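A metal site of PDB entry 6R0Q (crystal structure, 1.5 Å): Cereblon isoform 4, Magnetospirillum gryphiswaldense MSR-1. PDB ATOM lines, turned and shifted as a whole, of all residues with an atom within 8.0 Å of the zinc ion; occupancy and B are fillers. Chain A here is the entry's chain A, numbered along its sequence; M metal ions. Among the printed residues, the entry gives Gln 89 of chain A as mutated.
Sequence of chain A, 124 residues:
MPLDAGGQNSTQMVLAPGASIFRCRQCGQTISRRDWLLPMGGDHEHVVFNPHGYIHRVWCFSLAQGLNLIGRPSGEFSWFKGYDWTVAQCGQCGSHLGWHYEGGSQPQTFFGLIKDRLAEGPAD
OE1 of Gln 92 sits close to SG of Cys 27 (3.3 Å). The side-chain sulfur (SG) of Cys 27 sits close to the backbone NH (N) of Gln 29 (3.5 Å). The side-chain sulfur of Cys 24 lies close to the backbone NH of Gln 26 (3.5 Å). O of Gln 29 is in hydrogen-bond range of N of Cys 24, 2.8 Å away. The backbone NH (N) of Ser 95 lies close to the side-chain sulfur (SG) of Cys 93, 3.5 Å away. O of Ser 95 is in hydrogen-bond range of N of Cys 90 (2.8 Å). N of Gln 92 lies close to SG of Cys 90 (3.4 Å). The side-chain sulfur (SG) of Cys 90 lies close to the side-chain amide oxygen (OE1) of Gln 29 (3.4 Å).
The zinc ion is bound by SG of Cys 27, SG of Cys 24, SG of Cys 93 and SG of Cys 90.
Of the 21 residues printed, 4 come within 4 Å of the zinc ion.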
ATOM      1  N   ARG A  23      27.533 -13.462  24.267  1.00  0.00           N
ATOM      2  CA  ARG A  23      27.801 -14.665  23.475  1.00  0.00           C
ATOM      3  C   ARG A  23      26.524 -15.198  22.919  1.00  0.00           C
ATOM      4  O   ARG A  23      25.421 -15.008  23.460  1.00  0.00           O
ATOM      5  CB  ARG A  23      28.435 -15.691  24.385  1.00  0.00           C
ATOM      6  CG  ARG A  23      29.785 -15.262  24.926  1.00  0.00           C
ATOM      7  CD  ARG A  23      30.412 -16.358  25.808  1.00  0.00           C
ATOM      8  NE  ARG A  23      31.760 -15.954  26.176  1.00  0.00           N
ATOM      9  CZ  ARG A  23      32.062 -15.144  27.190  1.00  0.00           C
ATOM     10  NH1 ARG A  23      31.132 -14.685  28.157  1.00  0.00           N
ATOM     11  NH2 ARG A  23      33.396 -14.845  27.287  1.00  0.00           N
ATOM     12  N   CYS A  24      26.650 -15.946  21.835  1.00  0.00           N
ATOM     13  CA  CYS A  24      25.477 -16.736  21.431  1.00  0.00           C
ATOM     14  C   CYS A  24      24.967 -17.705  22.512  1.00  0.00           C
ATOM     15  O   CYS A  24      25.798 -18.468  23.058  1.00  0.00           O
ATOM     16  CB  CYS A  24      25.958 -17.565  20.202  1.00  0.00           C
ATOM     17  SG  CYS A  24      24.664 -18.691  19.533  1.00  0.00           S
ATOM     18  N   ARG A  25      23.706 -17.710  22.832  1.00  0.00           N
ATOM     19  CA  ARG A  25      23.254 -18.543  23.908  1.00  0.00           C
ATOM     20  C   ARG A  25      23.371 -19.974  23.520  1.00  0.00           C
ATOM     21  O   ARG A  25      23.723 -20.842  24.353  1.00  0.00           O
ATOM     22  CB  ARG A  25      21.857 -18.171  24.295  1.00  0.00           C
ATOM     23  CG  ARG A  25      21.349 -19.063  25.473  1.00  0.00           C
ATOM     24  CD  ARG A  25      19.908 -18.738  25.826  1.00  0.00           C
ATOM     25  NE  ARG A  25      19.729 -17.353  26.277  1.00  0.00           N
ATOM     26  CZ  ARG A  25      20.089 -16.838  27.468  1.00  0.00           C
ATOM     27  NH1 ARG A  25      19.876 -15.607  27.821  1.00  0.00           N
ATOM     28  NH2 ARG A  25      20.699 -17.633  28.340  1.00  0.00           N
ATOM     29  N   GLN A  26      23.122 -20.291  22.235  1.00  0.00           N
ATOM     30  CA  GLN A  26      23.155 -21.710  21.769  1.00  0.00           C
ATOM     31  C   GLN A  26      24.576 -22.270  21.751  1.00  0.00           C
ATOM     32  O   GLN A  26      24.682 -23.494  22.172  1.00  0.00           O
ATOM     33  CB  GLN A  26      22.523 -21.754  20.391  1.00  0.00           C
ATOM     34  CG  GLN A  26      20.994 -21.638  20.502  1.00  0.00           C
ATOM     35  CD  GLN A  26      20.572 -23.123  20.806  1.00  0.00           C
ATOM     36  OE1 GLN A  26      19.918 -23.421  21.737  1.00  0.00           O
ATOM     37  NE2 GLN A  26      21.054 -23.998  20.023  1.00  0.00           N
ATOM     38  N   CYS A  27      25.596 -21.542  21.381  1.00  0.00           N
ATOM     39  CA  CYS A  27      26.919 -22.150  21.283  1.00  0.00           C
ATOM     40  C   CYS A  27      28.030 -21.538  22.042  1.00  0.00           C
ATOM     41  O   CYS A  27      29.138 -22.141  22.122  1.00  0.00           O
ATOM     42  CB  CYS A  27      27.337 -22.338  19.908  1.00  0.00           C
ATOM     43  SG  CYS A  27      27.823 -20.805  19.032  1.00  0.00           S
ATOM     44  N   GLY A  28      27.873 -20.317  22.503  1.00  0.00           N
ATOM     45  CA  GLY A  28      28.922 -19.671  23.206  1.00  0.00           C
ATOM     46  C   GLY A  28      29.856 -18.788  22.406  1.00  0.00           C
ATOM     47  O   GLY A  28      30.734 -18.224  22.964  1.00  0.00           O
ATOM     48  N   GLN A  29      29.651 -18.686  21.121  1.00  0.00           N
ATOM     49  CA  GLN A  29      30.483 -17.810  20.309  1.00  0.00           C
ATOM     50  C   GLN A  29      30.370 -16.328  20.773  1.00  0.00           C
ATOM     51  O   GLN A  29      29.328 -15.880  21.013  1.00  0.00           O
ATOM     52  CB  GLN A  29      30.110 -17.831  18.810  1.00  0.00           C
ATOM     53  CG  GLN A  29      31.159 -17.095  18.002  1.00  0.00           C
ATOM     54  CD  GLN A  29      30.953 -16.957  16.559  1.00  0.00           C
ATOM     55  OE1 GLN A  29      29.878 -16.963  16.071  1.00  0.00           O
ATOM     56  NE2 GLN A  29      31.996 -16.680  15.888  1.00  0.00           N
ATOM     57  N   THR A  30      31.487 -15.645  20.847  1.00  0.00           N
ATOM     58  CA  THR A  30      31.501 -14.250  21.209  1.00  0.00           C
ATOM     59  C   THR A  30      30.892 -13.446  20.048  1.00  0.00           C
ATOM     60  O   THR A  30      31.288 -13.616  18.928  1.00  0.00           O
ATOM     61  CB  THR A  30      32.933 -13.789  21.445  1.00  0.00           C
ATOM     62  OG1 THR A  30      33.399 -14.393  22.633  1.00  0.00           O
ATOM     63  CG2 THR A  30      32.972 -12.307  21.661  1.00  0.00           C
ATOM     64  N   ILE A  31      29.930 -12.594  20.394  1.00  0.00           N
ATOM     65  CA  ILE A  31      29.232 -11.792  19.420  1.00  0.00           C
ATOM     66  C   ILE A  31      29.439 -10.314  19.593  1.00  0.00           C
ATOM     67  O   ILE A  31      29.761  -9.570  18.666  1.00  0.00           O
ATOM     68  CB  ILE A  31      27.732 -12.112  19.344  1.00  0.00           C
ATOM     69  CG1 ILE A  31      27.432 -13.578  19.147  1.00  0.00           C
ATOM     70  CG2 ILE A  31      26.942 -11.263  18.403  1.00  0.00           C
ATOM     71  CD1 ILE A  31      27.865 -14.185  17.852  1.00  0.00           C
ATOM     72  N   GLY A  66      31.309 -12.435  14.409  1.00  0.00           N
ATOM     73  CA  GLY A  66      30.870 -13.798  14.405  1.00  0.00           C
ATOM     74  C   GLY A  66      29.533 -14.128  13.764  1.00  0.00           C
ATOM     75  O   GLY A  66      28.979 -15.125  14.170  1.00  0.00           O
ATOM     76  N   LEU A  67      29.016 -13.180  13.016  1.00  0.00           N
ATOM     77  CA  LEU A  67      27.666 -13.317  12.387  1.00  0.00           C
ATOM     78  C   LEU A  67      27.774 -13.494  10.906  1.00  0.00           C
ATOM     79  O   LEU A  67      28.792 -13.038  10.274  1.00  0.00           O
ATOM     80  CB  LEU A  67      26.862 -12.101  12.656  1.00  0.00           C
ATOM     81  CG  LEU A  67      26.611 -11.802  14.099  1.00  0.00           C
ATOM     82  CD1 LEU A  67      25.998 -10.396  14.309  1.00  0.00           C
ATOM     83  CD2 LEU A  67      25.672 -12.791  14.640  1.00  0.00           C
ATOM     84  N   GLN A  89      22.719 -14.555  11.362  1.00  0.00           N
ATOM     85  CA  GLN A  89      22.832 -15.765  12.167  1.00  0.00           C
ATOM     86  C   GLN A  89      24.167 -15.878  12.790  1.00  0.00           C
ATOM     87  O   GLN A  89      25.143 -15.371  12.251  1.00  0.00           O
ATOM     88  CB  GLN A  89      22.719 -17.007  11.220  1.00  0.00           C
ATOM     89  CG  GLN A  89      21.376 -17.302  10.778  1.00  0.00           C
ATOM     90  CD  GLN A  89      21.304 -18.543   9.835  1.00  0.00           C
ATOM     91  OE1 GLN A  89      20.171 -18.825   9.489  1.00  0.00           O
ATOM     92  NE2 GLN A  89      22.389 -19.229   9.490  1.00  0.00           N
ATOM     93  N   CYS A  90      24.278 -16.632  13.900  1.00  0.00           N
ATOM     94  CA  CYS A  90      25.568 -16.983  14.487  1.00  0.00           C
ATOM     95  C   CYS A  90      26.349 -17.771  13.395  1.00  0.00           C
ATOM     96  O   CYS A  90      25.857 -18.737  12.768  1.00  0.00           O
ATOM     97  CB  CYS A  90      25.362 -17.808  15.705  1.00  0.00           C
ATOM     98  SG  CYS A  90      26.869 -18.453  16.406  1.00  0.00           S
ATOM     99  N   GLY A  91      27.580 -17.318  13.200  1.00  0.00           N
ATOM    100  CA  GLY A  91      28.446 -17.945  12.203  1.00  0.00           C
ATOM    101  C   GLY A  91      29.014 -19.253  12.701  1.00  0.00           C
ATOM    102  O   GLY A  91      29.577 -19.953  11.801  1.00  0.00           O
ATOM    103  N   GLN A  92      28.818 -19.641  13.902  1.00  0.00           N
ATOM    104  CA  GLN A  92      29.313 -20.920  14.407  1.00  0.00           C
ATOM    105  C   GLN A  92      28.212 -21.935  14.394  1.00  0.00           C
ATOM    106  O   GLN A  92      28.469 -23.060  14.098  1.00  0.00           O
ATOM    107  CB  GLN A  92      29.897 -20.839  15.763  1.00  0.00           C
ATOM    108  CG  GLN A  92      30.348 -22.164  16.288  1.00  0.00           C
ATOM    109  CD  GLN A  92      31.292 -22.088  17.422  1.00  0.00           C
ATOM    110  OE1 GLN A  92      31.052 -21.610  18.669  1.00  0.00           O
ATOM    111  NE2 GLN A  92      32.519 -22.531  17.037  1.00  0.00           N
ATOM    112  N   CYS A  93      26.999 -21.622  14.836  1.00  0.00           N
ATOM    113  CA  CYS A  93      25.923 -22.610  15.042  1.00  0.00           C
ATOM    114  C   CYS A  93      24.678 -22.347  14.282  1.00  0.00           C
ATOM    115  O   CYS A  93      23.682 -23.167  14.324  1.00  0.00           O
ATOM    116  CB  CYS A  93      25.533 -22.843  16.486  1.00  0.00           C
ATOM    117  SG  CYS A  93      24.522 -21.480  17.187  1.00  0.00           S
ATOM    118  N   GLY A  94      24.614 -21.183  13.613  1.00  0.00           N
ATOM    119  CA  GLY A  94      23.434 -20.835  12.838  1.00  0.00           C
ATOM    120  C   GLY A  94      22.213 -20.310  13.572  1.00  0.00           C
ATOM    121  O   GLY A  94      21.188 -20.027  12.902  1.00  0.00           O
ATOM    122  N   SER A  95      22.269 -20.138  14.859  1.00  0.00           N
ATOM    123  CA  SER A  95      21.193 -19.532  15.604  1.00  0.00           C
ATOM    124  C   SER A  95      20.844 -18.172  15.047  1.00  0.00           C
ATOM    125  O   SER A  95      21.732 -17.392  14.687  1.00  0.00           O
ATOM    126  CB  SER A  95      21.591 -19.367  17.099  1.00  0.00           C
ATOM    127  OG  SER A  95      20.498 -18.862  17.856  1.00  0.00           O
ATOM    128  N   HIS A  96      19.549 -17.898  14.926  1.00  0.00           N
ATOM    129  CA  HIS A  96      19.123 -16.555  14.464  1.00  0.00           C
ATOM    130  C   HIS A  96      19.226 -15.527  15.550  1.00  0.00           C
ATOM    131  O   HIS A  96      18.356 -15.443  16.403  1.00  0.00           O
ATOM    132  CB  HIS A  96      17.749 -16.645  13.896  1.00  0.00           C
ATOM    133  CG  HIS A  96      17.275 -15.321  13.379  1.00  0.00           C
ATOM    134  ND1 HIS A  96      15.928 -15.096  13.104  1.00  0.00           N
ATOM    135  CD2 HIS A  96      17.934 -14.233  13.008  1.00  0.00           C
ATOM    136  CE1 HIS A  96      15.823 -13.807  12.689  1.00  0.00           C
ATOM    137  NE2 HIS A  96      17.016 -13.273  12.633  1.00  0.00           N
ATOM    138  N   LEU A  97      20.276 -14.760  15.577  1.00  0.00           N
ATOM    139  CA  LEU A  97      20.565 -13.870  16.665  1.00  0.00           C
ATOM    140  C   LEU A  97      19.936 -12.502  16.457  1.00  0.00           C
ATOM    141  O   LEU A  97      19.782 -11.795  17.414  1.00  0.00           O
ATOM    142  CB  LEU A  97      22.066 -13.774  16.888  1.00  0.00           C
ATOM    143  CG  LEU A  97      22.763 -15.073  17.303  1.00  0.00           C
ATOM    144  CD1 LEU A  97      24.177 -14.766  17.572  1.00  0.00           C
ATOM    145  CD2 LEU A  97      22.058 -15.790  18.493  1.00  0.00           C
ATOM    146  N   ARG A 117      18.416 -14.487  22.976  1.00  0.00           N
ATOM    147  CA  ARG A 117      19.211 -15.413  22.230  1.00  0.00           C
ATOM    148  C   ARG A 117      20.720 -15.194  22.460  1.00  0.00           C
ATOM    149  O   ARG A 117      21.547 -15.889  21.875  1.00  0.00           O
ATOM    150  CB  ARG A 117      18.910 -15.381  20.715  1.00  0.00           C
ATOM    151  CG  ARG A 117      17.463 -15.853  20.527  1.00  0.00           C
ATOM    152  CD  ARG A 117      17.082 -15.994  19.130  1.00  0.00           C
ATOM    153  NE  ARG A 117      15.622 -16.324  18.967  1.00  0.00           N
ATOM    154  CZ  ARG A 117      14.939 -16.138  17.916  1.00  0.00           C
ATOM    155  NH1 ARG A 117      15.501 -15.915  16.742  1.00  0.00           N
ATOM    156  NH2 ARG A 117      13.566 -16.340  17.942  1.00  0.00           N
HETATM  157 ZN    ZN M   1      25.966 -19.881  18.049  1.00  0.00          ZN
